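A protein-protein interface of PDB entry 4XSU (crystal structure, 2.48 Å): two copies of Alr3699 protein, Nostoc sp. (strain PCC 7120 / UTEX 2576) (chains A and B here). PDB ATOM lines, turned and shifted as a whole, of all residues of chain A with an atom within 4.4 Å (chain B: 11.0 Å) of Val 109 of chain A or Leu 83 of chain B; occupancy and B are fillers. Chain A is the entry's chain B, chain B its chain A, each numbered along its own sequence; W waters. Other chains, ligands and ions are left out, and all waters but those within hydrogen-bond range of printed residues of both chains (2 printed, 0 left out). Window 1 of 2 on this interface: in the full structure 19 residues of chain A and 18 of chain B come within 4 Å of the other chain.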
ATOM      1  N   ASN A  62      -4.431  -3.516 -29.903  1.00  0.00           N
ATOM      2  CA  ASN A  62      -5.418  -3.497 -30.987  1.00  0.00           C
ATOM      3  C   ASN A  62      -4.734  -3.723 -32.362  1.00  0.00           C
ATOM      4  O   ASN A  62      -5.255  -3.296 -33.395  1.00  0.00           O
ATOM      5  CB  ASN A  62      -6.217  -2.180 -30.951  1.00  0.00           C
ATOM      6  CG  ASN A  62      -7.690  -2.365 -31.313  1.00  0.00           C
ATOM      7  OD1 ASN A  62      -8.293  -3.413 -31.063  1.00  0.00           O
ATOM      8  ND2 ASN A  62      -8.285  -1.328 -31.883  1.00  0.00           N
ATOM      9  N   ALA A  84     -11.973  -4.468 -34.396  1.00  0.00           N
ATOM     10  CA  ALA A  84     -11.438  -4.236 -33.043  1.00  0.00           C
ATOM     11  C   ALA A  84     -10.654  -5.484 -32.560  1.00  0.00           C
ATOM     12  O   ALA A  84     -11.184  -6.337 -31.841  1.00  0.00           O
ATOM     13  CB  ALA A  84     -12.564  -3.903 -32.078  1.00  0.00           C
ATOM     14  N   GLN A 105     -14.436   0.831 -17.059  1.00  0.00           N
ATOM     15  CA  GLN A 105     -15.449   1.063 -18.072  1.00  0.00           C
ATOM     16  C   GLN A 105     -15.136   0.427 -19.449  1.00  0.00           C
ATOM     17  O   GLN A 105     -15.947  -0.325 -19.986  1.00  0.00           O
ATOM     18  CB  GLN A 105     -15.697   2.563 -18.227  1.00  0.00           C
ATOM     19  CG  GLN A 105     -16.702   3.096 -17.220  1.00  0.00           C
ATOM     20  CD  GLN A 105     -17.032   4.540 -17.480  1.00  0.00           C
ATOM     21  OE1 GLN A 105     -17.477   4.883 -18.571  1.00  0.00           O
ATOM     22  NE2 GLN A 105     -16.797   5.406 -16.490  1.00  0.00           N
ATOM     23  N   LYS A 106     -13.973   0.724 -20.011  1.00  0.00           N
ATOM     24  CA  LYS A 106     -13.571   0.086 -21.243  1.00  0.00           C
ATOM     25  C   LYS A 106     -13.480  -1.395 -21.060  1.00  0.00           C
ATOM     26  O   LYS A 106     -13.754  -2.139 -21.986  1.00  0.00           O
ATOM     27  CB  LYS A 106     -12.246   0.614 -21.747  1.00  0.00           C
ATOM     28  CG  LYS A 106     -12.361   2.041 -22.219  1.00  0.00           C
ATOM     29  CD  LYS A 106     -11.078   2.483 -22.888  1.00  0.00           C
ATOM     30  CE  LYS A 106     -11.112   3.979 -23.150  1.00  0.00           C
ATOM     31  NZ  LYS A 106      -9.818   4.445 -23.710  1.00  0.00           N
ATOM     32  N   ALA A 107     -13.111  -1.855 -19.874  1.00  0.00           N
ATOM     33  CA  ALA A 107     -13.049  -3.286 -19.691  1.00  0.00           C
ATOM     34  C   ALA A 107     -14.419  -3.885 -19.632  1.00  0.00           C
ATOM     35  O   ALA A 107     -14.563  -5.086 -19.816  1.00  0.00           O
ATOM     36  CB  ALA A 107     -12.279  -3.649 -18.445  1.00  0.00           C
ATOM     37  N   LEU A 108     -15.428  -3.073 -19.323  1.00  0.00           N
ATOM     38  CA  LEU A 108     -16.799  -3.578 -19.338  1.00  0.00           C
ATOM     39  C   LEU A 108     -17.294  -3.778 -20.799  1.00  0.00           C
ATOM     40  O   LEU A 108     -17.897  -4.796 -21.145  1.00  0.00           O
ATOM     41  CB  LEU A 108     -17.720  -2.624 -18.599  1.00  0.00           C
ATOM     42  CG  LEU A 108     -19.183  -3.020 -18.637  1.00  0.00           C
ATOM     43  CD1 LEU A 108     -19.398  -4.437 -18.162  1.00  0.00           C
ATOM     44  CD2 LEU A 108     -19.983  -2.067 -17.786  1.00  0.00           C
ATOM     45  N   VAL A 109     -17.025  -2.790 -21.641  1.00  0.00           N
ATOM     46  CA  VAL A 109     -17.367  -2.886 -23.054  1.00  0.00           C
ATOM     47  C   VAL A 109     -16.840  -4.201 -23.635  1.00  0.00           C
ATOM     48  O   VAL A 109     -17.597  -5.042 -24.138  1.00  0.00           O
ATOM     49  CB  VAL A 109     -16.805  -1.697 -23.843  1.00  0.00           C
ATOM     50  CG1 VAL A 109     -17.162  -1.836 -25.307  1.00  0.00           C
ATOM     51  CG2 VAL A 109     -17.351  -0.389 -23.298  1.00  0.00           C
ATOM     52  N   VAL A 110     -15.539  -4.392 -23.503  1.00  0.00           N
ATOM     53  CA  VAL A 110     -14.879  -5.555 -24.065  1.00  0.00           C
ATOM     54  C   VAL A 110     -15.367  -6.817 -23.424  1.00  0.00           C
ATOM     55  O   VAL A 110     -15.604  -7.821 -24.097  1.00  0.00           O
ATOM     56  CB  VAL A 110     -13.368  -5.471 -23.854  1.00  0.00           C
ATOM     57  CG1 VAL A 110     -12.684  -6.754 -24.304  1.00  0.00           C
ATOM     58  CG2 VAL A 110     -12.804  -4.276 -24.600  1.00  0.00           C
ATOM     59  N   GLY A 111     -15.507  -6.768 -22.110  1.00  0.00           N
ATOM     60  CA  GLY A 111     -15.859  -7.950 -21.343  1.00  0.00           C
ATOM     61  C   GLY A 111     -17.294  -8.375 -21.544  1.00  0.00           C
ATOM     62  O   GLY A 111     -17.608  -9.568 -21.456  1.00  0.00           O
ATOM     63  N   ALA A 112     -18.169  -7.402 -21.756  1.00  0.00           N
ATOM     64  CA  ALA A 112     -19.536  -7.697 -22.176  1.00  0.00           C
ATOM     65  C   ALA A 112     -19.531  -8.472 -23.524  1.00  0.00           C
ATOM     66  O   ALA A 112     -20.219  -9.486 -23.690  1.00  0.00           O
ATOM     67  CB  ALA A 112     -20.333  -6.415 -22.299  1.00  0.00           C
ATOM     68  N   ILE A 113     -18.729  -8.003 -24.470  1.00  0.00           N
ATOM     69  CA  ILE A 113     -18.666  -8.638 -25.772  1.00  0.00           C
ATOM     70  C   ILE A 113     -18.135 -10.058 -25.656  1.00  0.00           C
ATOM     71  O   ILE A 113     -18.781 -10.987 -26.110  1.00  0.00           O
ATOM     72  CB  ILE A 113     -17.849  -7.797 -26.757  1.00  0.00           C
ATOM     73  CG1 ILE A 113     -18.616  -6.502 -27.084  1.00  0.00           C
ATOM     74  CG2 ILE A 113     -17.584  -8.594 -28.011  1.00  0.00           C
ATOM     75  CD1 ILE A 113     -17.774  -5.407 -27.696  1.00  0.00           C
ATOM     76  N   VAL A 142     -23.763   3.768 -21.967  1.00  0.00           N
ATOM     77  CA  VAL A 142     -23.131   2.508 -22.310  1.00  0.00           C
ATOM     78  C   VAL A 142     -22.936   1.590 -21.111  1.00  0.00           C
ATOM     79  O   VAL A 142     -23.283   0.387 -21.169  1.00  0.00           O
ATOM     80  CB  VAL A 142     -21.790   2.722 -23.043  1.00  0.00           C
ATOM     81  CG1 VAL A 142     -21.048   1.403 -23.220  1.00  0.00           C
ATOM     82  CG2 VAL A 142     -22.042   3.359 -24.405  1.00  0.00           C
ATOM     83  N   LEU A 146     -24.779  -1.980 -20.783  1.00  0.00           N
ATOM     84  CA  LEU A 146     -24.022  -3.247 -20.836  1.00  0.00           C
ATOM     85  C   LEU A 146     -24.088  -3.990 -19.511  1.00  0.00           C
ATOM     86  O   LEU A 146     -24.119  -5.229 -19.482  1.00  0.00           O
ATOM     87  CB  LEU A 146     -22.556  -3.027 -21.223  1.00  0.00           C
ATOM     88  CG  LEU A 146     -22.362  -2.409 -22.609  1.00  0.00           C
ATOM     89  CD1 LEU A 146     -20.913  -2.056 -22.868  1.00  0.00           C
ATOM     90  CD2 LEU A 146     -22.858  -3.378 -23.658  1.00  0.00           C
ATOM     91  N   THR B  61     -12.046   5.349 -41.558  1.00  0.00           N
ATOM     92  CA  THR B  61     -10.902   4.570 -41.137  1.00  0.00           C
ATOM     93  C   THR B  61     -10.943   4.386 -39.626  1.00  0.00           C
ATOM     94  O   THR B  61     -11.663   5.093 -38.894  1.00  0.00           O
ATOM     95  CB  THR B  61      -9.594   5.310 -41.465  1.00  0.00           C
ATOM     96  OG1 THR B  61      -9.690   6.663 -40.986  1.00  0.00           O
ATOM     97  CG2 THR B  61      -9.350   5.342 -42.964  1.00  0.00           C
ATOM     98  N   ASN B  62     -10.132   3.446 -39.169  1.00  0.00           N
ATOM     99  CA  ASN B  62      -9.949   3.202 -37.756  1.00  0.00           C
ATOM    100  C   ASN B  62      -8.717   3.944 -37.169  1.00  0.00           C
ATOM    101  O   ASN B  62      -8.279   3.627 -36.066  1.00  0.00           O
ATOM    102  CB  ASN B  62      -9.848   1.690 -37.517  1.00  0.00           C
ATOM    103  CG  ASN B  62     -10.520   1.261 -36.232  1.00  0.00           C
ATOM    104  OD1 ASN B  62     -11.553   1.811 -35.828  1.00  0.00           O
ATOM    105  ND2 ASN B  62      -9.941   0.279 -35.577  1.00  0.00           N
ATOM    106  N   GLN B  63      -8.219   4.954 -37.877  1.00  0.00           N
ATOM    107  CA  GLN B  63      -7.202   5.853 -37.328  1.00  0.00           C
ATOM    108  C   GLN B  63      -7.811   6.745 -36.240  1.00  0.00           C
ATOM    109  O   GLN B  63      -8.993   7.081 -36.305  1.00  0.00           O
ATOM    110  CB  GLN B  63      -6.590   6.712 -38.435  1.00  0.00           C
ATOM    111  CG  GLN B  63      -6.270   5.948 -39.709  1.00  0.00           C
ATOM    112  CD  GLN B  63      -5.228   4.868 -39.494  1.00  0.00           C
ATOM    113  OE1 GLN B  63      -4.976   4.448 -38.365  1.00  0.00           O
ATOM    114  NE2 GLN B  63      -4.615   4.413 -40.581  1.00  0.00           N
ATOM    115  N   PRO B  64      -7.014   7.126 -35.240  1.00  0.00           N
ATOM    116  CA  PRO B  64      -7.541   7.949 -34.116  1.00  0.00           C
ATOM    117  C   PRO B  64      -8.084   9.347 -34.481  1.00  0.00           C
ATOM    118  O   PRO B  64      -8.027   9.748 -35.632  1.00  0.00           O
ATOM    119  CB  PRO B  64      -6.326   8.091 -33.197  1.00  0.00           C
ATOM    120  CG  PRO B  64      -5.408   6.964 -33.567  1.00  0.00           C
ATOM    121  CD  PRO B  64      -5.609   6.728 -35.026  1.00  0.00           C
ATOM    122  N   ILE B  65      -8.560  10.091 -33.480  1.00  0.00           N
ATOM    123  CA  ILE B  65      -9.337  11.339 -33.672  1.00  0.00           C
ATOM    124  C   ILE B  65     -10.613  11.025 -34.437  1.00  0.00           C
ATOM    125  O   ILE B  65     -11.578  10.545 -33.853  1.00  0.00           O
ATOM    126  CB  ILE B  65      -8.549  12.499 -34.362  1.00  0.00           C
ATOM    127  CG1 ILE B  65      -7.601  13.176 -33.351  1.00  0.00           C
ATOM    128  CG2 ILE B  65      -9.506  13.535 -34.974  1.00  0.00           C
ATOM    129  CD1 ILE B  65      -6.876  14.408 -33.871  1.00  0.00           C
ATOM    130  N   PHE B  77     -18.938  12.367 -28.055  1.00  0.00           N
ATOM    131  CA  PHE B  77     -18.962  10.924 -27.806  1.00  0.00           C
ATOM    132  C   PHE B  77     -18.490  10.625 -26.374  1.00  0.00           C
ATOM    133  O   PHE B  77     -19.229  10.851 -25.413  1.00  0.00           O
ATOM    134  CB  PHE B  77     -18.121  10.171 -28.870  1.00  0.00           C
ATOM    135  CG  PHE B  77     -18.312   8.667 -28.861  1.00  0.00           C
ATOM    136  CD1 PHE B  77     -19.437   8.100 -29.435  1.00  0.00           C
ATOM    137  CD2 PHE B  77     -17.361   7.812 -28.298  1.00  0.00           C
ATOM    138  CE1 PHE B  77     -19.626   6.719 -29.439  1.00  0.00           C
ATOM    139  CE2 PHE B  77     -17.546   6.427 -28.304  1.00  0.00           C
ATOM    140  CZ  PHE B  77     -18.680   5.880 -28.876  1.00  0.00           C
ATOM    141  N   GLY B  78     -17.251  10.162 -26.237  1.00  0.00           N
ATOM    142  CA  GLY B  78     -16.704   9.733 -24.965  1.00  0.00           C
ATOM    143  C   GLY B  78     -15.320   9.153 -25.191  1.00  0.00           C
ATOM    144  O   GLY B  78     -14.792   9.170 -26.314  1.00  0.00           O
ATOM    145  N   SER B  79     -14.736   8.629 -24.124  1.00  0.00           N
ATOM    146  CA  SER B  79     -13.408   8.024 -24.192  1.00  0.00           C
ATOM    147  C   SER B  79     -13.446   6.643 -24.863  1.00  0.00           C
ATOM    148  O   SER B  79     -12.433   6.170 -25.393  1.00  0.00           O
ATOM    149  CB  SER B  79     -12.817   7.915 -22.783  1.00  0.00           C
ATOM    150  OG  SER B  79     -13.672   7.171 -21.936  1.00  0.00           O
ATOM    151  N   LEU B  80     -14.622   6.023 -24.865  1.00  0.00           N
ATOM    152  CA  LEU B  80     -14.788   4.651 -25.376  1.00  0.00           C
ATOM    153  C   LEU B  80     -14.378   4.509 -26.844  1.00  0.00           C
ATOM    154  O   LEU B  80     -14.025   3.416 -27.276  1.00  0.00           O
ATOM    155  CB  LEU B  80     -16.235   4.174 -25.170  1.00  0.00           C
ATOM    156  CG  LEU B  80     -16.749   4.271 -23.718  1.00  0.00           C
ATOM    157  CD1 LEU B  80     -18.270   4.265 -23.661  1.00  0.00           C
ATOM    158  CD2 LEU B  80     -16.164   3.166 -22.842  1.00  0.00           C
ATOM    159  N   GLY B  81     -14.404   5.622 -27.581  1.00  0.00           N
ATOM    160  CA  GLY B  81     -13.949   5.695 -28.975  1.00  0.00           C
ATOM    161  C   GLY B  81     -12.558   5.170 -29.282  1.00  0.00           C
ATOM    162  O   GLY B  81     -12.331   4.697 -30.374  1.00  0.00           O
ATOM    163  N   GLN B  82     -11.630   5.238 -28.329  1.00  0.00           N
ATOM    164  CA  GLN B  82     -10.270   4.708 -28.532  1.00  0.00           C
ATOM    165  C   GLN B  82     -10.245   3.213 -28.827  1.00  0.00           C
ATOM    166  O   GLN B  82      -9.323   2.725 -29.494  1.00  0.00           O
ATOM    167  CB  GLN B  82      -9.396   4.958 -27.307  1.00  0.00           C
ATOM    168  CG  GLN B  82      -9.202   6.429 -27.009  1.00  0.00           C
ATOM    169  CD  GLN B  82      -7.936   6.719 -26.225  1.00  0.00           C
ATOM    170  OE1 GLN B  82      -7.288   5.810 -25.700  1.00  0.00           O
ATOM    171  NE2 GLN B  82      -7.579   7.996 -26.138  1.00  0.00           N
ATOM    172  N   LEU B  83     -11.236   2.493 -28.301  1.00  0.00           N
ATOM    173  CA  LEU B  83     -11.394   1.074 -28.593  1.00  0.00           C
ATOM    174  C   LEU B  83     -11.600   0.815 -30.082  1.00  0.00           C
ATOM    175  O   LEU B  83     -11.134  -0.198 -30.588  1.00  0.00           O
ATOM    176  CB  LEU B  83     -12.585   0.486 -27.826  1.00  0.00           C
ATOM    177  CG  LEU B  83     -12.397   0.313 -26.324  1.00  0.00           C
ATOM    178  CD1 LEU B  83     -13.715   0.040 -25.608  1.00  0.00           C
ATOM    179  CD2 LEU B  83     -11.397  -0.806 -26.053  1.00  0.00           C
ATOM    180  N   ALA B  84     -12.295   1.739 -30.752  1.00  0.00           N
ATOM    181  CA  ALA B  84     -12.746   1.567 -32.137  1.00  0.00           C
ATOM    182  C   ALA B  84     -13.143   2.908 -32.773  1.00  0.00           C
ATOM    183  O   ALA B  84     -14.317   3.305 -32.756  1.00  0.00           O
ATOM    184  CB  ALA B  84     -13.919   0.607 -32.173  1.00  0.00           C
ATOM    185  N   PRO B  85     -12.163   3.618 -33.333  1.00  0.00           N
ATOM    186  CA  PRO B  85     -12.432   4.978 -33.814  1.00  0.00           C
ATOM    187  C   PRO B  85     -13.450   5.068 -34.952  1.00  0.00           C
ATOM    188  O   PRO B  85     -14.292   5.992 -34.996  1.00  0.00           O
ATOM    189  CB  PRO B  85     -11.052   5.445 -34.286  1.00  0.00           C
ATOM    190  CG  PRO B  85     -10.094   4.692 -33.429  1.00  0.00           C
ATOM    191  CD  PRO B  85     -10.718   3.335 -33.257  1.00  0.00           C
ATOM    192  N   LEU B  86     -13.345   4.115 -35.873  1.00  0.00           N
ATOM    193  CA  LEU B  86     -14.294   3.976 -36.974  1.00  0.00           C
ATOM    194  C   LEU B  86     -15.704   4.094 -36.450  1.00  0.00           C
ATOM    195  O   LEU B  86     -16.491   4.916 -36.927  1.00  0.00           O
ATOM    196  CB  LEU B  86     -14.104   2.624 -37.672  1.00  0.00           C
ATOM    197  CG  LEU B  86     -14.781   2.437 -39.041  1.00  0.00           C
ATOM    198  CD1 LEU B  86     -13.871   1.676 -40.001  1.00  0.00           C
ATOM    199  CD2 LEU B  86     -16.114   1.731 -38.888  1.00  0.00           C
ATOM    200  N   VAL B  87     -16.008   3.284 -35.446  1.00  0.00           N
ATOM    201  CA  VAL B  87     -17.328   3.305 -34.822  1.00  0.00           C
ATOM    202  C   VAL B  87     -17.679   4.715 -34.317  1.00  0.00           C
ATOM    203  O   VAL B  87     -18.791   5.228 -34.558  1.00  0.00           O
ATOM    204  CB  VAL B  87     -17.417   2.295 -33.664  1.00  0.00           C
ATOM    205  CG1 VAL B  87     -18.768   2.393 -32.966  1.00  0.00           C
ATOM    206  CG2 VAL B  87     -17.159   0.880 -34.163  1.00  0.00           C
ATOM    207  N   ALA B  88     -16.725   5.346 -33.637  1.00  0.00           N
ATOM    208  CA  ALA B  88     -16.955   6.678 -33.065  1.00  0.00           C
ATOM    209  C   ALA B  88     -17.285   7.676 -34.150  1.00  0.00           C
ATOM    210  O   ALA B  88     -18.249   8.430 -34.031  1.00  0.00           O
ATOM    211  CB  ALA B  88     -15.735   7.146 -32.271  1.00  0.00           C
ATOM    212  N   LYS B  89     -16.476   7.667 -35.205  1.00  0.00           N
ATOM    213  CA  LYS B  89     -16.713   8.531 -36.370  1.00  0.00           C
ATOM    214  C   LYS B  89     -18.102   8.323 -36.976  1.00  0.00           C
ATOM    215  O   LYS B  89     -18.825   9.288 -37.276  1.00  0.00           O
ATOM    216  CB  LYS B  89     -15.676   8.251 -37.434  1.00  0.00           C
ATOM    217  CG  LYS B  89     -14.261   8.591 -37.005  1.00  0.00           C
ATOM    218  CD  LYS B  89     -13.224   7.882 -37.860  1.00  0.00           C
ATOM    219  CE  LYS B  89     -11.829   8.377 -37.532  1.00  0.00           C
ATOM    220  NZ  LYS B  89     -10.801   7.639 -38.304  1.00  0.00           N
ATOM    221  N   VAL B 109     -22.975  -4.330 -37.402  1.00  0.00           N
ATOM    222  CA  VAL B 109     -22.295  -4.125 -36.134  1.00  0.00           C
ATOM    223  C   VAL B 109     -22.120  -2.635 -35.834  1.00  0.00           C
ATOM    224  O   VAL B 109     -22.559  -2.127 -34.800  1.00  0.00           O
ATOM    225  CB  VAL B 109     -20.923  -4.809 -36.130  1.00  0.00           C
ATOM    226  CG1 VAL B 109     -20.198  -4.498 -34.847  1.00  0.00           C
ATOM    227  CG2 VAL B 109     -21.092  -6.314 -36.253  1.00  0.00           C
ATOM    228  N   VAL B 110     -21.510  -1.932 -36.759  1.00  0.00           N
ATOM    229  CA  VAL B 110     -21.226  -0.532 -36.537  1.00  0.00           C
ATOM    230  C   VAL B 110     -22.516   0.249 -36.484  1.00  0.00           C
ATOM    231  O   VAL B 110     -22.663   1.146 -35.672  1.00  0.00           O
ATOM    232  CB  VAL B 110     -20.300   0.038 -37.625  1.00  0.00           C
ATOM    233  CG1 VAL B 110     -20.117   1.543 -37.482  1.00  0.00           C
ATOM    234  CG2 VAL B 110     -18.942  -0.660 -37.585  1.00  0.00           C
ATOM    235  N   ILE B 113     -24.463  -0.130 -33.139  1.00  0.00           N
ATOM    236  CA  ILE B 113     -23.877   0.727 -32.149  1.00  0.00           C
ATOM    237  C   ILE B 113     -24.360   2.143 -32.349  1.00  0.00           C
ATOM    238  O   ILE B 113     -24.958   2.733 -31.452  1.00  0.00           O
ATOM    239  CB  ILE B 113     -22.355   0.629 -32.214  1.00  0.00           C
ATOM    240  CG1 ILE B 113     -21.923  -0.778 -31.785  1.00  0.00           C
ATOM    241  CG2 ILE B 113     -21.701   1.665 -31.315  1.00  0.00           C
ATOM    242  CD1 ILE B 113     -20.448  -1.056 -32.025  1.00  0.00           C
ATOM    243  N   PHE B 116     -27.997   2.862 -31.532  1.00  0.00           N
ATOM    244  CA  PHE B 116     -28.265   3.031 -30.108  1.00  0.00           C
ATOM    245  C   PHE B 116     -27.792   4.380 -29.568  1.00  0.00           C
ATOM    246  O   PHE B 116     -28.541   5.127 -28.938  1.00  0.00           O
ATOM    247  CB  PHE B 116     -27.577   1.937 -29.316  1.00  0.00           C
ATOM    248  CG  PHE B 116     -27.773   2.072 -27.852  1.00  0.00           C
ATOM    249  CD1 PHE B 116     -29.003   1.798 -27.291  1.00  0.00           C
ATOM    250  CD2 PHE B 116     -26.748   2.516 -27.044  1.00  0.00           C
ATOM    251  CE1 PHE B 116     -29.201   1.933 -25.938  1.00  0.00           C
ATOM    252  CE2 PHE B 116     -26.941   2.652 -25.694  1.00  0.00           C
ATOM    253  CZ  PHE B 116     -28.167   2.362 -25.142  1.00  0.00           C
ATOM    254  N   ILE B 117     -26.541   4.695 -29.830  1.00  0.00           N
ATOM    255  CA  ILE B 117     -25.973   5.901 -29.288  1.00  0.00           C
ATOM    256  C   ILE B 117     -26.595   7.152 -29.903  1.00  0.00           C
ATOM    257  O   ILE B 117     -26.943   8.086 -29.185  1.00  0.00           O
ATOM    258  CB  ILE B 117     -24.471   5.927 -29.474  1.00  0.00           C
ATOM    259  CG1 ILE B 117     -23.846   4.758 -28.710  1.00  0.00           C
ATOM    260  CG2 ILE B 117     -23.930   7.245 -28.994  1.00  0.00           C
ATOM    261  CD1 ILE B 117     -22.343   4.626 -28.905  1.00  0.00           C
HETATM  262  O   HOH W   1     -10.803  -1.174 -33.003  1.00  0.00           O
HETATM  263  O   HOH W   2      -9.926   6.865 -23.901  1.00  0.00           O
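5 positions are printed for both chains.
Of the 6 pairs that touch across the chains among the printed residues, none has its exchanged pair printed and touching as well.
No residue of chain B comes within 4 Å of Ala 84 of chain A.
No residue of chain B comes within 4 Å of Ala 107 of chain A.
No residue of chain B comes within 4 Å of Leu 108 of chain A.
Of chain B, only Leu 80 (3.8 Å) and Leu 83 (3.9 Å) come within 4 Å of Val 109 of chain A.
No residue of chain B comes within 4 Å of Ala 112 of chain A.
No residue of chain B comes within 4 Å of Ile 113 of chain A.
Of the printed residues of chain B, Val 142 of chain A touches Leu 80.
Of the printed residues of chain A, Ser 79 of chain B touches Lys 106.
Of the printed residues of chain A, Leu 80 of chain B touches Val 109 (3.8 Å) and Val 142 (3.9 Å).
Of the printed residues of chain A, Leu 83 of chain B touches Asn 62 (3.3 Å) and Val 109 (3.9 Å).
The nearest printed residue of chain A that does not touch Leu 83 of chain B is Val 110 of chain A (4.02 Å).
The nearest printed residue of chain B that does not touch Val 142 of chain A is Ile 117 of chain B (4.7 Å).
NZ of Lys 106 of chain A is in hydrogen-bond range of OE1 of Gln 82 of chain B, at 3.5 Å.
ND2 of Asn 62 of chain A sits at hydrogen-bond distance from O of Leu 83 of chain B, 3.3 Å away.
Printed residues of chain A that touch a printed residue of chain B: Asn 62, Lys 106, Val 109 and Val 142.
Hydrophobic or aromatic side chains of chain A that line the printed part of chain B: Val 109 and Val 142.
Hydrophobic or aromatic side chains of chain B within 4 Å of the printed part of chain A: Leu 80 and Leu 83.
Among the printed residues, 6 pairs touch across the chains.
Ser 79 of chain B touches Lys 106 of chain A.
CD2 of Leu 80 of chain B touches CG2 of Val 109 of chain A (3.8 Å).
CG1 of Val 109 of chain A touches CD1 of Leu 83 of chain B (3.9 Å).
Leu 80 of chain B touches Val 142 of chain A.
Water W2 lies within hydrogen-bond range of the side-chain amino group (NZ) of Lys 106 of chain A (2.4 Å), the backbone carbonyl oxygen (O) of Ser 79 of chain B (3.0 Å) and the side-chain amide oxygen (OE1) of Gln 82 of chain B (3.4 Å).
Water W1 lies within hydrogen-bond range of the backbone carbonyl oxygen (O) of Leu 83 of chain B (2.6 Å), the side-chain amide nitrogen (ND2) of Asn 62 of chain A (2.8 Å) and the side-chain amide nitrogen (ND2) of Asn 62 of chain B (3.1 Å).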
